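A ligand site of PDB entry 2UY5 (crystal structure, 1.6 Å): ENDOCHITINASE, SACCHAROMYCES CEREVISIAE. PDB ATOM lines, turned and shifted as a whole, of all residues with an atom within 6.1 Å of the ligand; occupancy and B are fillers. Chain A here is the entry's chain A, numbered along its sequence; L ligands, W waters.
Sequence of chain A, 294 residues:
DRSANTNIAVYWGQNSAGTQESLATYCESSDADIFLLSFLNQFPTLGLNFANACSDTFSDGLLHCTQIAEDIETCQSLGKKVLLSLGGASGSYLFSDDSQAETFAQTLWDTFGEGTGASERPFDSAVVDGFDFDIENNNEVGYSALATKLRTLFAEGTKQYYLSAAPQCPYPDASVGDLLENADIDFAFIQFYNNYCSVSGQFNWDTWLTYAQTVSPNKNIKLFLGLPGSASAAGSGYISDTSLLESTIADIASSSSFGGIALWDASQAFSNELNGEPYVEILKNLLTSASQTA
The backbone NH of Ala 89 lies within hydrogen-bond range of the side-chain carboxylate of Glu 136. O of Ala 262 lies within hydrogen-bond range of N of Leu 227. OH of Tyr 193 sits at hydrogen-bond distance from OE1 of Gln 191 (3.4 Å). N of Gln 191 sits at hydrogen-bond distance from O of Pro 167 (2.9 Å). The side-chain hydroxyl of Tyr 11 sits at hydrogen-bond distance from the side-chain carboxylate of Asp 132 (2.6 Å). The backbone NH (N) of Ala 262 is in hydrogen-bond range of the backbone carbonyl oxygen (O) of Leu 225 (3.0 Å). The backbone carbonyl oxygen (O) of Ala 166 sits at hydrogen-bond distance from the side-chain amide nitrogen (NE2) of Gln 191 (3.1 Å). O of Asp 134 lies within hydrogen-bond range of N of Gly 88 (3.0 Å).
OH of Tyr 193 lies within hydrogen-bond range of N4 of the ligand, at 2.7 Å. The side-chain amide oxygen (OE1) of Gln 191 lies close to a nitrogen (N1) of the ligand (3.4 Å). A nitrogen (N3) of the ligand sits close to the side-chain carboxylate (OE2) of Glu 136, 3.2 Å away. A nitrogen (N2) of the ligand lies close to the side-chain carboxylate of Asp 134 (2.6 Å).
Residues that only touch the ligand: Phe 189 (3.2 Å), Tyr 11 (3.3 Å), Trp 264 (3.4 Å), Phe 39 (3.6 Å), Ala 262 (3.7 Å) and Gly 226 (3.8 Å). Hydrophobic or aromatic side chains that line the ligand: Tyr 11, Phe 39, Phe 189, Tyr 193, Ala 262 and Trp 264. Of the 22 residues printed, 10 come within 4 Å of the ligand.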
ATOM      1  N   TYR A  11       9.892 -15.216   7.704  1.00  0.00           N
ATOM      2  CA  TYR A  11       9.450 -14.501   8.932  1.00  0.00           C
ATOM      3  C   TYR A  11       7.984 -14.097   8.734  1.00  0.00           C
ATOM      4  O   TYR A  11       7.618 -13.703   7.641  1.00  0.00           O
ATOM      5  CB  TYR A  11      10.354 -13.269   9.159  1.00  0.00           C
ATOM      6  CG  TYR A  11      11.650 -13.753   9.763  1.00  0.00           C
ATOM      7  CD1 TYR A  11      12.661 -14.328   8.942  1.00  0.00           C
ATOM      8  CD2 TYR A  11      11.844 -13.692  11.125  1.00  0.00           C
ATOM      9  CE1 TYR A  11      13.807 -14.859   9.520  1.00  0.00           C
ATOM     10  CE2 TYR A  11      13.017 -14.180  11.722  1.00  0.00           C
ATOM     11  CZ  TYR A  11      14.006 -14.770  10.914  1.00  0.00           C
ATOM     12  OH  TYR A  11      15.129 -15.316  11.529  1.00  0.00           O
ATOM     13  N   PHE A  39       7.231 -10.977  16.711  1.00  0.00           N
ATOM     14  CA  PHE A  39       8.318 -11.395  17.615  1.00  0.00           C
ATOM     15  C   PHE A  39       7.858 -11.498  19.069  1.00  0.00           C
ATOM     16  O   PHE A  39       6.940 -10.818  19.500  1.00  0.00           O
ATOM     17  CB  PHE A  39       9.463 -10.371  17.659  1.00  0.00           C
ATOM     18  CG  PHE A  39      10.221 -10.253  16.361  1.00  0.00           C
ATOM     19  CD1 PHE A  39      11.103 -11.263  15.959  1.00  0.00           C
ATOM     20  CD2 PHE A  39      10.089  -9.112  15.568  1.00  0.00           C
ATOM     21  CE1 PHE A  39      11.808 -11.140  14.760  1.00  0.00           C
ATOM     22  CE2 PHE A  39      10.788  -8.988  14.328  1.00  0.00           C
ATOM     23  CZ  PHE A  39      11.673 -10.006  13.955  1.00  0.00           C
ATOM     24  N   GLY A  88      13.986  -8.422  17.380  1.00  0.00           N
ATOM     25  CA  GLY A  88      13.439  -7.376  16.579  1.00  0.00           C
ATOM     26  C   GLY A  88      13.894  -5.979  16.971  1.00  0.00           C
ATOM     27  O   GLY A  88      14.721  -5.783  17.889  1.00  0.00           O
ATOM     28  N   ALA A  89      13.347  -4.991  16.269  1.00  0.00           N
ATOM     29  CA  ALA A  89      13.791  -3.602  16.338  1.00  0.00           C
ATOM     30  C   ALA A  89      13.418  -2.865  17.630  1.00  0.00           C
ATOM     31  O   ALA A  89      13.791  -1.712  17.829  1.00  0.00           O
ATOM     32  CB  ALA A  89      13.247  -2.861  15.132  1.00  0.00           C
ATOM     33  N   ASP A 132      13.923 -18.844  17.465  1.00  0.00           N
ATOM     34  CA  ASP A 132      14.874 -18.141  16.624  1.00  0.00           C
ATOM     35  C   ASP A 132      15.411 -16.959  17.402  1.00  0.00           C
ATOM     36  O   ASP A 132      14.657 -16.320  18.171  1.00  0.00           O
ATOM     37  CB  ASP A 132      14.154 -17.640  15.382  1.00  0.00           C
ATOM     38  CG  ASP A 132      15.043 -16.792  14.455  1.00  0.00           C
ATOM     39  OD1 ASP A 132      16.120 -17.301  14.053  1.00  0.00           O
ATOM     40  OD2 ASP A 132      14.619 -15.654  14.080  1.00  0.00           O
ATOM     41  N   ASP A 134      16.652 -13.452  16.822  1.00  0.00           N
ATOM     42  CA  ASP A 134      16.752 -12.361  15.865  1.00  0.00           C
ATOM     43  C   ASP A 134      17.067 -11.097  16.672  1.00  0.00           C
ATOM     44  O   ASP A 134      16.310 -10.126  16.702  1.00  0.00           O
ATOM     45  CB  ASP A 134      15.489 -12.256  15.016  1.00  0.00           C
ATOM     46  CG  ASP A 134      15.637 -11.295  13.827  1.00  0.00           C
ATOM     47  OD1 ASP A 134      16.695 -10.625  13.676  1.00  0.00           O
ATOM     48  OD2 ASP A 134      14.709 -11.226  13.000  1.00  0.00           O
ATOM     49  N   GLU A 136      18.909  -7.740  17.833  1.00  0.00           N
ATOM     50  CA  GLU A 136      19.337  -6.559  17.060  1.00  0.00           C
ATOM     51  C   GLU A 136      19.949  -5.408  17.882  1.00  0.00           C
ATOM     52  O   GLU A 136      20.147  -4.298  17.365  1.00  0.00           O
ATOM     53  CB  GLU A 136      18.154  -5.989  16.278  1.00  0.00           C
ATOM     54  CG  GLU A 136      17.562  -6.875  15.236  1.00  0.00           C
ATOM     55  CD  GLU A 136      16.391  -6.195  14.546  1.00  0.00           C
ATOM     56  OE1 GLU A 136      16.422  -4.972  14.367  1.00  0.00           O
ATOM     57  OE2 GLU A 136      15.408  -6.889  14.227  1.00  0.00           O
ATOM     58  N   ALA A 166      19.443 -15.208  13.459  1.00  0.00           N
ATOM     59  CA  ALA A 166      19.253 -14.367  12.270  1.00  0.00           C
ATOM     60  C   ALA A 166      20.306 -13.254  12.232  1.00  0.00           C
ATOM     61  O   ALA A 166      19.964 -12.038  12.358  1.00  0.00           O
ATOM     62  CB  ALA A 166      17.857 -13.752  12.277  1.00  0.00           C
ATOM     63  N   PRO A 167      21.603 -13.631  12.043  1.00  0.00           N
ATOM     64  CA  PRO A 167      22.639 -12.604  11.917  1.00  0.00           C
ATOM     65  C   PRO A 167      22.441 -11.768  10.650  1.00  0.00           C
ATOM     66  O   PRO A 167      21.815 -12.240   9.685  1.00  0.00           O
ATOM     67  CB  PRO A 167      23.930 -13.409  11.774  1.00  0.00           C
ATOM     68  CG  PRO A 167      23.479 -14.736  11.186  1.00  0.00           C
ATOM     69  CD  PRO A 167      22.150 -14.997  11.856  1.00  0.00           C
ATOM     70  N   PHE A 189      19.875 -17.960   9.583  1.00  0.00           N
ATOM     71  CA  PHE A 189      19.141 -17.206   8.603  1.00  0.00           C
ATOM     72  C   PHE A 189      19.882 -15.874   8.418  1.00  0.00           C
ATOM     73  O   PHE A 189      19.623 -14.893   9.106  1.00  0.00           O
ATOM     74  CB  PHE A 189      17.688 -16.989   9.068  1.00  0.00           C
ATOM     75  CG  PHE A 189      16.931 -18.262   9.388  1.00  0.00           C
ATOM     76  CD1 PHE A 189      16.789 -19.257   8.438  1.00  0.00           C
ATOM     77  CD2 PHE A 189      16.330 -18.440  10.632  1.00  0.00           C
ATOM     78  CE1 PHE A 189      16.088 -20.451   8.752  1.00  0.00           C
ATOM     79  CE2 PHE A 189      15.623 -19.595  10.958  1.00  0.00           C
ATOM     80  CZ  PHE A 189      15.483 -20.606   9.999  1.00  0.00           C
ATOM     81  N   ILE A 190      20.841 -15.868   7.475  1.00  0.00           N
ATOM     82  CA  ILE A 190      21.801 -14.756   7.340  1.00  0.00           C
ATOM     83  C   ILE A 190      21.249 -13.688   6.396  1.00  0.00           C
ATOM     84  O   ILE A 190      20.877 -13.977   5.239  1.00  0.00           O
ATOM     85  CB  ILE A 190      23.162 -15.270   6.822  1.00  0.00           C
ATOM     86  CG1 ILE A 190      23.688 -16.397   7.714  1.00  0.00           C
ATOM     87  CG2 ILE A 190      24.189 -14.120   6.710  1.00  0.00           C
ATOM     88  CD1 ILE A 190      24.639 -17.361   6.992  1.00  0.00           C
ATOM     89  N   GLN A 191      21.153 -12.451   6.900  1.00  0.00           N
ATOM     90  CA  GLN A 191      20.608 -11.345   6.098  1.00  0.00           C
ATOM     91  C   GLN A 191      21.664 -10.784   5.152  1.00  0.00           C
ATOM     92  O   GLN A 191      22.480  -9.951   5.548  1.00  0.00           O
ATOM     93  CB  GLN A 191      20.078 -10.250   7.019  1.00  0.00           C
ATOM     94  CG  GLN A 191      19.038 -10.742   8.021  1.00  0.00           C
ATOM     95  CD  GLN A 191      18.714  -9.705   9.044  1.00  0.00           C
ATOM     96  OE1 GLN A 191      18.410  -8.553   8.697  1.00  0.00           O
ATOM     97  NE2 GLN A 191      18.769 -10.069  10.301  1.00  0.00           N
ATOM     98  N   TYR A 193      21.448  -8.572   2.954  1.00  0.00           N
ATOM     99  CA  TYR A 193      20.814  -7.351   2.483  1.00  0.00           C
ATOM    100  C   TYR A 193      21.030  -6.260   3.521  1.00  0.00           C
ATOM    101  O   TYR A 193      21.485  -6.550   4.611  1.00  0.00           O
ATOM    102  CB  TYR A 193      19.325  -7.589   2.150  1.00  0.00           C
ATOM    103  CG  TYR A 193      18.447  -8.035   3.309  1.00  0.00           C
ATOM    104  CD1 TYR A 193      18.248  -9.402   3.593  1.00  0.00           C
ATOM    105  CD2 TYR A 193      17.802  -7.082   4.102  1.00  0.00           C
ATOM    106  CE1 TYR A 193      17.424  -9.793   4.653  1.00  0.00           C
ATOM    107  CE2 TYR A 193      16.978  -7.458   5.146  1.00  0.00           C
ATOM    108  CZ  TYR A 193      16.804  -8.803   5.430  1.00  0.00           C
ATOM    109  OH  TYR A 193      15.970  -9.132   6.456  1.00  0.00           O
ATOM    110  N   ASN A 194      20.748  -5.004   3.152  1.00  0.00           N
ATOM    111  CA  ASN A 194      21.006  -3.840   4.018  1.00  0.00           C
ATOM    112  C   ASN A 194      22.451  -3.720   4.483  1.00  0.00           C
ATOM    113  O   ASN A 194      22.709  -3.149   5.536  1.00  0.00           O
ATOM    114  CB  ASN A 194      20.081  -3.839   5.237  1.00  0.00           C
ATOM    115  CG  ASN A 194      18.640  -3.579   4.894  1.00  0.00           C
ATOM    116  OD1 ASN A 194      18.327  -3.113   3.784  1.00  0.00           O
ATOM    117  ND2 ASN A 194      17.745  -3.851   5.843  1.00  0.00           N
ATOM    118  N   LEU A 225      20.359 -18.451   2.795  1.00  0.00           N
ATOM    119  CA  LEU A 225      20.460 -17.192   2.081  1.00  0.00           C
ATOM    120  C   LEU A 225      19.256 -16.293   2.393  1.00  0.00           C
ATOM    121  O   LEU A 225      18.156 -16.491   1.857  1.00  0.00           O
ATOM    122  CB  LEU A 225      20.573 -17.461   0.556  1.00  0.00           C
ATOM    123  CG  LEU A 225      20.682 -16.305  -0.423  1.00  0.00           C
ATOM    124  CD1 LEU A 225      22.025 -15.567  -0.229  1.00  0.00           C
ATOM    125  CD2 LEU A 225      20.576 -16.798  -1.869  1.00  0.00           C
ATOM    126  N   GLY A 226      19.466 -15.293   3.253  1.00  0.00           N
ATOM    127  CA  GLY A 226      18.395 -14.413   3.732  1.00  0.00           C
ATOM    128  C   GLY A 226      18.226 -13.217   2.816  1.00  0.00           C
ATOM    129  O   GLY A 226      19.196 -12.498   2.546  1.00  0.00           O
ATOM    130  N   LEU A 227      16.995 -12.998   2.365  1.00  0.00           N
ATOM    131  CA  LEU A 227      16.677 -11.978   1.354  1.00  0.00           C
ATOM    132  C   LEU A 227      15.418 -11.151   1.660  1.00  0.00           C
ATOM    133  O   LEU A 227      14.510 -11.647   2.310  1.00  0.00           O
ATOM    134  CB  LEU A 227      16.505 -12.635  -0.037  1.00  0.00           C
ATOM    135  CG  LEU A 227      17.701 -13.335  -0.682  1.00  0.00           C
ATOM    136  CD1 LEU A 227      17.265 -13.963  -1.973  1.00  0.00           C
ATOM    137  CD2 LEU A 227      18.914 -12.397  -0.915  1.00  0.00           C
ATOM    138  N   ALA A 233      10.736  -4.179   1.163  1.00  0.00           N
ATOM    139  CA  ALA A 233      10.878  -4.944   2.400  1.00  0.00           C
ATOM    140  C   ALA A 233      12.104  -4.494   3.182  1.00  0.00           C
ATOM    141  O   ALA A 233      12.239  -4.670   4.351  1.00  0.00           O
ATOM    142  CB  ALA A 233      10.977  -6.306   2.098  1.00  0.00           C
ATOM    143  N   ALA A 234      12.982  -3.848   2.453  1.00  0.00           N
ATOM    144  CA  ALA A 234      14.326  -3.427   2.891  1.00  0.00           C
ATOM    145  C   ALA A 234      14.886  -2.230   2.141  1.00  0.00           C
ATOM    146  O   ALA A 234      14.579  -2.064   1.018  1.00  0.00           O
ATOM    147  CB  ALA A 234      15.243  -4.518   2.824  1.00  0.00           C
ATOM    148  N   ALA A 262      15.878 -17.815   3.184  1.00  0.00           N
ATOM    149  CA  ALA A 262      15.034 -17.231   4.249  1.00  0.00           C
ATOM    150  C   ALA A 262      14.574 -15.851   3.794  1.00  0.00           C
ATOM    151  O   ALA A 262      15.372 -15.065   3.248  1.00  0.00           O
ATOM    152  CB  ALA A 262      15.843 -17.113   5.577  1.00  0.00           C
ATOM    153  N   LEU A 263      13.294 -15.532   4.020  1.00  0.00           N
ATOM    154  CA  LEU A 263      12.707 -14.298   3.466  1.00  0.00           C
ATOM    155  C   LEU A 263      12.138 -13.358   4.533  1.00  0.00           C
ATOM    156  O   LEU A 263      11.409 -13.813   5.414  1.00  0.00           O
ATOM    157  CB  LEU A 263      11.624 -14.642   2.425  1.00  0.00           C
ATOM    158  CG  LEU A 263      12.179 -15.290   1.147  1.00  0.00           C
ATOM    159  CD1 LEU A 263      11.093 -16.090   0.455  1.00  0.00           C
ATOM    160  CD2 LEU A 263      12.797 -14.249   0.227  1.00  0.00           C
ATOM    161  N   TRP A 264      12.437 -12.059   4.416  1.00  0.00           N
ATOM    162  CA  TRP A 264      11.806 -11.028   5.237  1.00  0.00           C
ATOM    163  C   TRP A 264      10.833 -10.246   4.312  1.00  0.00           C
ATOM    164  O   TRP A 264      11.282  -9.535   3.430  1.00  0.00           O
ATOM    165  CB  TRP A 264      12.839 -10.019   5.797  1.00  0.00           C
ATOM    166  CG  TRP A 264      12.133  -8.993   6.618  1.00  0.00           C
ATOM    167  CD1 TRP A 264      11.749  -7.734   6.217  1.00  0.00           C
ATOM    168  CD2 TRP A 264      11.687  -9.162   7.951  1.00  0.00           C
ATOM    169  NE1 TRP A 264      11.073  -7.102   7.248  1.00  0.00           N
ATOM    170  CE2 TRP A 264      11.032  -7.959   8.324  1.00  0.00           C
ATOM    171  CE3 TRP A 264      11.792 -10.202   8.898  1.00  0.00           C
ATOM    172  CZ2 TRP A 264      10.472  -7.771   9.608  1.00  0.00           C
ATOM    173  CZ3 TRP A 264      11.217 -10.024  10.174  1.00  0.00           C
ATOM    174  CH2 TRP A 264      10.564  -8.815  10.510  1.00  0.00           C
HETATM  175  C1  LIG L   1      16.963 -13.271   8.370  1.00  0.00           C
HETATM  176  C2  LIG L   1      16.904 -13.806   7.136  1.00  0.00           C
HETATM  177  C3  LIG L   1      15.811 -13.337   6.510  1.00  0.00           C
HETATM  178  O1  LIG L   1      15.168 -12.509   7.382  1.00  0.00           O
HETATM  179  C4  LIG L   1      15.903 -12.466   8.519  1.00  0.00           C
HETATM  180  C5  LIG L   1      15.464 -11.612   9.717  1.00  0.00           C
HETATM  181  N1  LIG L   1      15.421 -10.184   9.221  1.00  0.00           N
HETATM  182  C6  LIG L   1      14.899  -9.190   9.927  1.00  0.00           C
HETATM  183  N2  LIG L   1      14.645  -9.348  11.226  1.00  0.00           N
HETATM  184  C7  LIG L   1      14.105  -8.356  11.944  1.00  0.00           C
HETATM  185  N3  LIG L   1      13.797  -7.161  11.425  1.00  0.00           N
HETATM  186  C8  LIG L   1      14.051  -6.929  10.134  1.00  0.00           C
HETATM  187  C9  LIG L   1      14.606  -7.949   9.347  1.00  0.00           C
HETATM  188  N4  LIG L   1      14.743  -7.446   8.123  1.00  0.00           N
HETATM  189  C10 LIG L   1      14.271  -6.182   8.115  1.00  0.00           C
HETATM  190  N5  LIG L   1      13.859  -5.858   9.343  1.00  0.00           N
HETATM  191  O   HOH W   1      12.092  -5.749  13.682  1.00  0.00           O
